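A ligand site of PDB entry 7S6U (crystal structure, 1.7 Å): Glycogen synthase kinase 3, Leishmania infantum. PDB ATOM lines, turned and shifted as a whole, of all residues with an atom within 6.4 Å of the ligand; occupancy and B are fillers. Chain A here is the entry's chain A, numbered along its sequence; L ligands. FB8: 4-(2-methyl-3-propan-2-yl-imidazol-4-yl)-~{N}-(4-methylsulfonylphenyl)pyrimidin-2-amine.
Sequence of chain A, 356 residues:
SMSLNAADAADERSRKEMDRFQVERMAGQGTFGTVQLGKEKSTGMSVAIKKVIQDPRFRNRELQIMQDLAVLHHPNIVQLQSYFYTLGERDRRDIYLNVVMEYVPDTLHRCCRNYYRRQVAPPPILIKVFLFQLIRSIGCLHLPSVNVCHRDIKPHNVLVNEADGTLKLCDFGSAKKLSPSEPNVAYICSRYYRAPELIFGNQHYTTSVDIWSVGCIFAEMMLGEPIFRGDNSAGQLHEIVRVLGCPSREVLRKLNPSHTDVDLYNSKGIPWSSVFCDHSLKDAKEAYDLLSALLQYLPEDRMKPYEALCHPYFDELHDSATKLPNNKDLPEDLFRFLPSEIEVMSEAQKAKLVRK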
ATOM      1  N   ALA A  27      36.139   0.835  -1.729  1.00  0.00           N
ATOM      2  CA  ALA A  27      35.660  -0.487  -1.364  1.00  0.00           C
ATOM      3  C   ALA A  27      34.662  -0.995  -2.400  1.00  0.00           C
ATOM      4  O   ALA A  27      34.714  -2.123  -2.818  1.00  0.00           O
ATOM      5  CB  ALA A  27      35.040  -0.482   0.008  1.00  0.00           C
ATOM      6  N   GLY A  28      33.728  -0.160  -2.784  1.00  0.00           N
ATOM      7  CA  GLY A  28      32.739  -0.551  -3.743  1.00  0.00           C
ATOM      8  C   GLY A  28      31.884   0.587  -4.255  1.00  0.00           C
ATOM      9  O   GLY A  28      31.704   1.564  -3.566  1.00  0.00           O
ATOM     10  N   GLN A  29      31.392   0.454  -5.474  1.00  0.00           N
ATOM     11  CA  GLN A  29      30.520   1.471  -6.025  1.00  0.00           C
ATOM     12  C   GLN A  29      29.360   0.836  -6.755  1.00  0.00           C
ATOM     13  O   GLN A  29      29.473  -0.273  -7.271  1.00  0.00           O
ATOM     14  CB  GLN A  29      31.254   2.477  -6.908  1.00  0.00           C
ATOM     15  CG  GLN A  29      32.345   1.950  -7.815  1.00  0.00           C
ATOM     16  CD  GLN A  29      33.050   3.083  -8.529  1.00  0.00           C
ATOM     17  OE1 GLN A  29      32.601   4.236  -8.476  1.00  0.00           O
ATOM     18  NE2 GLN A  29      34.152   2.767  -9.185  1.00  0.00           N
ATOM     19  N   PHE A  32      23.590   2.968  -5.242  1.00  0.00           N
ATOM     20  CA  PHE A  32      23.528   3.681  -3.928  1.00  0.00           C
ATOM     21  C   PHE A  32      24.542   4.832  -3.796  1.00  0.00           C
ATOM     22  O   PHE A  32      24.346   5.715  -2.940  1.00  0.00           O
ATOM     23  CB  PHE A  32      23.871   2.766  -2.744  1.00  0.00           C
ATOM     24  CG  PHE A  32      25.186   2.056  -2.886  1.00  0.00           C
ATOM     25  CD1 PHE A  32      26.379   2.579  -2.381  1.00  0.00           C
ATOM     26  CD2 PHE A  32      25.245   0.806  -3.483  1.00  0.00           C
ATOM     27  CE1 PHE A  32      27.576   1.907  -2.566  1.00  0.00           C
ATOM     28  CE2 PHE A  32      26.444   0.136  -3.651  1.00  0.00           C
ATOM     29  CZ  PHE A  32      27.609   0.687  -3.193  1.00  0.00           C
ATOM     30  N   VAL A  35      31.322   3.560  -1.633  1.00  0.00           N
ATOM     31  CA  VAL A  35      31.849   3.273  -0.304  1.00  0.00           C
ATOM     32  C   VAL A  35      33.350   3.210  -0.432  1.00  0.00           C
ATOM     33  O   VAL A  35      33.833   2.391  -1.186  1.00  0.00           O
ATOM     34  CB  VAL A  35      31.276   2.006   0.312  1.00  0.00           C
ATOM     35  CG1 VAL A  35      31.982   1.816   1.653  1.00  0.00           C
ATOM     36  CG2 VAL A  35      29.770   2.135   0.462  1.00  0.00           C
ATOM     37  N   VAL A  47      36.742   2.304   8.698  1.00  0.00           N
ATOM     38  CA  VAL A  47      35.376   2.888   8.493  1.00  0.00           C
ATOM     39  C   VAL A  47      34.996   2.752   7.027  1.00  0.00           C
ATOM     40  O   VAL A  47      35.875   2.733   6.165  1.00  0.00           O
ATOM     41  CB  VAL A  47      35.268   4.348   8.962  1.00  0.00           C
ATOM     42  CG1 VAL A  47      35.431   4.431  10.492  1.00  0.00           C
ATOM     43  CG2 VAL A  47      36.227   5.277   8.274  1.00  0.00           C
ATOM     44  N   ALA A  48      33.707   2.642   6.835  1.00  0.00           N
ATOM     45  CA  ALA A  48      33.077   2.779   5.492  1.00  0.00           C
ATOM     46  C   ALA A  48      32.571   4.210   5.344  1.00  0.00           C
ATOM     47  O   ALA A  48      31.770   4.688   6.188  1.00  0.00           O
ATOM     48  CB  ALA A  48      31.986   1.767   5.415  1.00  0.00           C
ATOM     49  N   LYS A  50      30.560   6.443   3.114  1.00  0.00           N
ATOM     50  CA  LYS A  50      29.577   6.243   2.029  1.00  0.00           C
ATOM     51  C   LYS A  50      29.044   7.569   1.517  1.00  0.00           C
ATOM     52  O   LYS A  50      28.473   8.312   2.268  1.00  0.00           O
ATOM     53  CB  LYS A  50      28.420   5.415   2.523  1.00  0.00           C
ATOM     54  CG  LYS A  50      27.311   5.321   1.486  1.00  0.00           C
ATOM     55  CD  LYS A  50      26.423   4.185   1.805  1.00  0.00           C
ATOM     56  CE  LYS A  50      25.250   4.419   2.686  1.00  0.00           C
ATOM     57  NZ  LYS A  50      24.220   3.358   2.427  1.00  0.00           N
ATOM     58  N   GLU A  62      18.231   7.744   5.201  1.00  0.00           N
ATOM     59  CA  GLU A  62      19.450   7.077   5.710  1.00  0.00           C
ATOM     60  C   GLU A  62      19.960   7.853   6.935  1.00  0.00           C
ATOM     61  O   GLU A  62      20.225   7.216   7.985  1.00  0.00           O
ATOM     62  CB  GLU A  62      20.501   6.904   4.631  1.00  0.00           C
ATOM     63  CG  GLU A  62      21.748   6.226   5.156  1.00  0.00           C
ATOM     64  CD  GLU A  62      22.465   5.258   4.253  1.00  0.00           C
ATOM     65  OE1 GLU A  62      22.607   5.576   3.049  1.00  0.00           O
ATOM     66  OE2 GLU A  62      22.927   4.193   4.774  1.00  0.00           O
ATOM     67  N   VAL A  78      24.989  -1.556  11.764  1.00  0.00           N
ATOM     68  CA  VAL A  78      26.122  -0.593  11.608  1.00  0.00           C
ATOM     69  C   VAL A  78      25.884   0.621  12.501  1.00  0.00           C
ATOM     70  O   VAL A  78      24.716   0.986  12.783  1.00  0.00           O
ATOM     71  CB  VAL A  78      26.311  -0.176  10.150  1.00  0.00           C
ATOM     72  CG1 VAL A  78      26.852  -1.324   9.363  1.00  0.00           C
ATOM     73  CG2 VAL A  78      25.020   0.363   9.555  1.00  0.00           C
ATOM     74  N   MET A 101      30.474   4.843   8.861  1.00  0.00           N
ATOM     75  CA  MET A 101      30.116   3.801   9.802  1.00  0.00           C
ATOM     76  C   MET A 101      31.281   2.815   9.856  1.00  0.00           C
ATOM     77  O   MET A 101      32.237   2.960   9.126  1.00  0.00           O
ATOM     78  CB  MET A 101      28.843   3.089   9.355  1.00  0.00           C
ATOM     79  CG  MET A 101      28.955   2.382   8.022  1.00  0.00           C
ATOM     80  SD  MET A 101      27.347   2.213   7.215  1.00  0.00           S
ATOM     81  CE  MET A 101      27.071   3.894   6.694  1.00  0.00           C
ATOM     82  N   GLU A 102      31.211   1.800  10.710  1.00  0.00           N
ATOM     83  CA  GLU A 102      32.340   0.897  10.764  1.00  0.00           C
ATOM     84  C   GLU A 102      32.389   0.061   9.503  1.00  0.00           C
ATOM     85  O   GLU A 102      31.366  -0.183   8.868  1.00  0.00           O
ATOM     86  CB  GLU A 102      32.335  -0.003  11.994  1.00  0.00           C
ATOM     87  CG  GLU A 102      31.223  -1.018  12.014  1.00  0.00           C
ATOM     88  CD  GLU A 102      29.969  -0.453  12.620  1.00  0.00           C
ATOM     89  OE1 GLU A 102      29.835   0.774  12.777  1.00  0.00           O
ATOM     90  OE2 GLU A 102      29.102  -1.259  12.940  1.00  0.00           O
ATOM     91  N   TYR A 103      33.586  -0.362   9.137  1.00  0.00           N
ATOM     92  CA  TYR A 103      33.721  -1.162   7.954  1.00  0.00           C
ATOM     93  C   TYR A 103      33.520  -2.642   8.189  1.00  0.00           C
ATOM     94  O   TYR A 103      34.027  -3.191   9.157  1.00  0.00           O
ATOM     95  CB  TYR A 103      35.092  -0.951   7.336  1.00  0.00           C
ATOM     96  CG  TYR A 103      35.323  -1.648   6.028  1.00  0.00           C
ATOM     97  CD1 TYR A 103      34.739  -1.165   4.861  1.00  0.00           C
ATOM     98  CD2 TYR A 103      36.144  -2.757   5.935  1.00  0.00           C
ATOM     99  CE1 TYR A 103      34.955  -1.793   3.651  1.00  0.00           C
ATOM    100  CE2 TYR A 103      36.360  -3.385   4.725  1.00  0.00           C
ATOM    101  CZ  TYR A 103      35.764  -2.898   3.589  1.00  0.00           C
ATOM    102  OH  TYR A 103      35.977  -3.518   2.390  1.00  0.00           O
ATOM    103  N   VAL A 104      32.758  -3.281   7.318  1.00  0.00           N
ATOM    104  CA  VAL A 104      32.596  -4.774   7.374  1.00  0.00           C
ATOM    105  C   VAL A 104      33.100  -5.345   6.045  1.00  0.00           C
ATOM    106  O   VAL A 104      32.808  -4.773   5.000  1.00  0.00           O
ATOM    107  CB  VAL A 104      31.149  -5.163   7.697  1.00  0.00           C
ATOM    108  CG1 VAL A 104      30.983  -6.674   7.838  1.00  0.00           C
ATOM    109  CG2 VAL A 104      30.546  -4.421   8.904  1.00  0.00           C
ATOM    110  N   PRO A 105      33.960  -6.375   6.048  1.00  0.00           N
ATOM    111  CA  PRO A 105      34.743  -6.649   4.845  1.00  0.00           C
ATOM    112  C   PRO A 105      33.974  -7.273   3.697  1.00  0.00           C
ATOM    113  O   PRO A 105      34.514  -7.309   2.626  1.00  0.00           O
ATOM    114  CB  PRO A 105      35.852  -7.613   5.267  1.00  0.00           C
ATOM    115  CG  PRO A 105      35.393  -8.134   6.584  1.00  0.00           C
ATOM    116  CD  PRO A 105      34.456  -7.115   7.196  1.00  0.00           C
ATOM    117  N   ASP A 106      32.767  -7.804   3.921  1.00  0.00           N
ATOM    118  CA  ASP A 106      32.080  -8.522   2.840  1.00  0.00           C
ATOM    119  C   ASP A 106      30.566  -8.354   2.904  1.00  0.00           C
ATOM    120  O   ASP A 106      30.043  -7.882   3.919  1.00  0.00           O
ATOM    121  CB  ASP A 106      32.484  -9.977   2.951  1.00  0.00           C
ATOM    122  CG  ASP A 106      32.419 -10.771   1.681  1.00  0.00           C
ATOM    123  OD1 ASP A 106      32.191 -10.164   0.600  1.00  0.00           O
ATOM    124  OD2 ASP A 106      32.566 -12.035   1.838  1.00  0.00           O
ATOM    125  N   THR A 107      29.921  -8.686   1.812  1.00  0.00           N
ATOM    126  CA  THR A 107      28.465  -8.796   1.794  1.00  0.00           C
ATOM    127  C   THR A 107      28.105 -10.279   1.914  1.00  0.00           C
ATOM    128  O   THR A 107      28.806 -11.184   1.451  1.00  0.00           O
ATOM    129  CB  THR A 107      27.793  -8.202   0.582  1.00  0.00           C
ATOM    130  OG1 THR A 107      28.113  -8.922  -0.610  1.00  0.00           O
ATOM    131  CG2 THR A 107      28.001  -6.706   0.473  1.00  0.00           C
ATOM    132  N   ARG A 110      28.229 -11.732  -1.650  1.00  0.00           N
ATOM    133  CA  ARG A 110      29.553 -12.141  -2.174  1.00  0.00           C
ATOM    134  C   ARG A 110      30.051 -13.374  -1.424  1.00  0.00           C
ATOM    135  O   ARG A 110      30.638 -14.302  -2.011  1.00  0.00           O
ATOM    136  CB  ARG A 110      30.518 -10.964  -2.039  1.00  0.00           C
ATOM    137  CG  ARG A 110      30.127  -9.827  -2.977  1.00  0.00           C
ATOM    138  CD  ARG A 110      30.930  -8.556  -2.759  1.00  0.00           C
ATOM    139  NE  ARG A 110      32.383  -8.736  -2.784  1.00  0.00           N
ATOM    140  CZ  ARG A 110      33.165  -8.526  -3.829  1.00  0.00           C
ATOM    141  NH1 ARG A 110      32.688  -8.130  -4.991  1.00  0.00           N
ATOM    142  NH2 ARG A 110      34.476  -8.677  -3.670  1.00  0.00           N
ATOM    143  N   HIS A 156      22.677  -8.143  -0.724  1.00  0.00           N
ATOM    144  CA  HIS A 156      23.629  -7.112  -1.055  1.00  0.00           C
ATOM    145  C   HIS A 156      23.811  -6.029   0.027  1.00  0.00           C
ATOM    146  O   HIS A 156      24.781  -5.297  -0.025  1.00  0.00           O
ATOM    147  CB  HIS A 156      23.265  -6.482  -2.392  1.00  0.00           C
ATOM    148  CG  HIS A 156      22.904  -7.479  -3.452  1.00  0.00           C
ATOM    149  ND1 HIS A 156      21.671  -8.076  -3.520  1.00  0.00           N
ATOM    150  CD2 HIS A 156      23.633  -7.983  -4.477  1.00  0.00           C
ATOM    151  CE1 HIS A 156      21.651  -8.915  -4.543  1.00  0.00           C
ATOM    152  NE2 HIS A 156      22.829  -8.876  -5.139  1.00  0.00           N
ATOM    153  N   ASN A 157      22.903  -5.941   1.001  1.00  0.00           N
ATOM    154  CA  ASN A 157      23.118  -4.963   2.082  1.00  0.00           C
ATOM    155  C   ASN A 157      23.109  -5.624   3.457  1.00  0.00           C
ATOM    156  O   ASN A 157      23.004  -4.934   4.486  1.00  0.00           O
ATOM    157  CB  ASN A 157      22.137  -3.794   2.039  1.00  0.00           C
ATOM    158  CG  ASN A 157      20.676  -4.209   2.051  1.00  0.00           C
ATOM    159  OD1 ASN A 157      20.329  -5.300   2.486  1.00  0.00           O
ATOM    160  ND2 ASN A 157      19.827  -3.374   1.462  1.00  0.00           N
ATOM    161  N   VAL A 158      23.341  -6.928   3.486  1.00  0.00           N
ATOM    162  CA  VAL A 158      23.648  -7.685   4.694  1.00  0.00           C
ATOM    163  C   VAL A 158      25.179  -7.869   4.666  1.00  0.00           C
ATOM    164  O   VAL A 158      25.696  -8.518   3.774  1.00  0.00           O
ATOM    165  CB  VAL A 158      22.917  -9.028   4.723  1.00  0.00           C
ATOM    166  CG1 VAL A 158      23.324  -9.841   5.956  1.00  0.00           C
ATOM    167  CG2 VAL A 158      21.427  -8.767   4.777  1.00  0.00           C
ATOM    168  N   LEU A 159      25.858  -7.323   5.631  1.00  0.00           N
ATOM    169  CA  LEU A 159      27.329  -7.312   5.701  1.00  0.00           C
ATOM    170  C   LEU A 159      27.767  -8.474   6.590  1.00  0.00           C
ATOM    171  O   LEU A 159      27.162  -8.721   7.712  1.00  0.00           O
ATOM    172  CB  LEU A 159      27.781  -5.987   6.319  1.00  0.00           C
ATOM    173  CG  LEU A 159      27.411  -4.736   5.545  1.00  0.00           C
ATOM    174  CD1 LEU A 159      27.710  -3.557   6.377  1.00  0.00           C
ATOM    175  CD2 LEU A 159      28.182  -4.643   4.259  1.00  0.00           C
ATOM    176  N   CYS A 170      22.794  -2.992   7.044  1.00  0.00           N
ATOM    177  CA  CYS A 170      23.043  -1.594   6.703  1.00  0.00           C
ATOM    178  C   CYS A 170      22.070  -1.088   5.657  1.00  0.00           C
ATOM    179  O   CYS A 170      21.040  -1.724   5.429  1.00  0.00           O
ATOM    180  CB  CYS A 170      24.467  -1.398   6.174  1.00  0.00           C
ATOM    181  SG  CYS A 170      24.773  -2.069   4.531  1.00  0.00           S
ATOM    182  N   ASP A 171      22.358   0.047   5.035  1.00  0.00           N
ATOM    183  CA  ASP A 171      21.545   0.545   3.912  1.00  0.00           C
ATOM    184  C   ASP A 171      20.121   0.930   4.299  1.00  0.00           C
ATOM    185  O   ASP A 171      19.181   0.306   3.841  1.00  0.00           O
ATOM    186  CB  ASP A 171      21.578  -0.488   2.797  1.00  0.00           C
ATOM    187  CG  ASP A 171      21.316   0.080   1.427  1.00  0.00           C
ATOM    188  OD1 ASP A 171      21.426   1.305   1.243  1.00  0.00           O
ATOM    189  OD2 ASP A 171      21.014  -0.744   0.524  1.00  0.00           O
HETATM  190  C4  FB8 L   1      27.746  -0.217   3.214  1.00  0.00           C
HETATM  191  C14 FB8 L   1      31.447  -2.782  -0.252  1.00  0.00           C
HETATM  192  C5  FB8 L   1      28.918  -0.738   3.944  1.00  0.00           C
HETATM  193  C6  FB8 L   1      29.067  -0.542   5.302  1.00  0.00           C
HETATM  194  C11 FB8 L   1      32.160  -4.975   0.442  1.00  0.00           C
HETATM  195  C7  FB8 L   1      30.195  -1.030   5.922  1.00  0.00           C
HETATM  196  C8  FB8 L   1      30.878  -1.911   3.978  1.00  0.00           C
HETATM  197  C9  FB8 L   1      31.805  -3.217   2.063  1.00  0.00           C
HETATM  198  C10 FB8 L   1      32.172  -4.534   1.766  1.00  0.00           C
HETATM  199  C12 FB8 L   1      31.772  -4.088  -0.551  1.00  0.00           C
HETATM  200  C13 FB8 L   1      30.984  -3.366  -3.121  1.00  0.00           C
HETATM  201  N1  FB8 L   1      25.920   1.032   2.712  1.00  0.00           N
HETATM  202  N2  FB8 L   1      31.116  -1.757   5.302  1.00  0.00           N
HETATM  203  C3  FB8 L   1      26.966   0.856   3.564  1.00  0.00           C
HETATM  204  N3  FB8 L   1      31.802  -2.695   3.366  1.00  0.00           N
HETATM  205  C1  FB8 L   1      25.240  -0.008   0.559  1.00  0.00           C
HETATM  206  C2  FB8 L   1      26.096   0.102   1.777  1.00  0.00           C
HETATM  207  S1  FB8 L   1      31.650  -4.657  -2.226  1.00  0.00           S
HETATM  208  O1  FB8 L   1      30.771  -5.777  -2.226  1.00  0.00           O
HETATM  209  O2  FB8 L   1      33.021  -5.005  -2.629  1.00  0.00           O
HETATM  210  C15 FB8 L   1      31.469  -2.351   1.055  1.00  0.00           C
HETATM  211  N4  FB8 L   1      29.839  -1.429   3.278  1.00  0.00           N
HETATM  212  N5  FB8 L   1      27.240  -0.632   1.970  1.00  0.00           N
HETATM  213  C16 FB8 L   1      27.664  -1.811   1.219  1.00  0.00           C
HETATM  214  C17 FB8 L   1      28.083  -1.473  -0.233  1.00  0.00           C
HETATM  215  C18 FB8 L   1      26.585  -2.904   1.281  1.00  0.00           C
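An oxygen (O1) of the ligand sits close to the guanidinium group (NE) of Arg 110 (3.4 Å). SG of Cys 170 sits close to N1 of the ligand. N2 of the ligand lies within hydrogen-bond range of N of Val 104, at 3.0 Å. The backbone carbonyl oxygen (O) of Val 104 lies within hydrogen-bond range of a nitrogen (N3) of the ligand (2.8 Å). NZ of Lys 50 lies within hydrogen-bond range of N1 of the ligand (2.9 Å).
NE of Arg 110 is in salt-bridge range of OD1 of Asp 106 (3.7 Å). The backbone NH of Ala 48 sits at hydrogen-bond distance from the backbone carbonyl oxygen of Met 101 (2.7 Å). The side-chain hydroxyl (OG1) of Thr 107 lies within hydrogen-bond range of the backbone NH (N) of Arg 110 (3.0 Å). The backbone NH of Cys 170 is in hydrogen-bond range of the backbone carbonyl oxygen of Asn 157. The backbone NH (N) of Ala 27 lies within hydrogen-bond range of the backbone carbonyl oxygen (O) of Val 35 (2.8 Å). The side-chain amino group (NZ) of Lys 50 is in salt-bridge range of the side-chain carboxylate (OE2) of Glu 62, 2.8 Å away. The backbone carbonyl oxygen of Gly 28 sits at hydrogen-bond distance from the backbone NH of Val 35 (2.8 Å). NZ of Lys 50 lies within salt-bridge range of OD1 of Asp 171 (3.7 Å).
O2 of the ligand sits close to O of Ala 27, 3.3 Å away. Residues that only touch the ligand: His 156, Glu 102, Tyr 103, Ala 48, Gly 28, Leu 159, Phe 32, Pro 105, Met 101, Asp 106 and Thr 107. 16 residues have an atom within 4 Å of the ligand: Ala 27, Gly 28, Phe 32, Ala 48, Lys 50, Met 101, Glu 102, Tyr 103, Val 104, Pro 105, Asp 106, Thr 107, Arg 110, His 156, Leu 159 and Cys 170.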
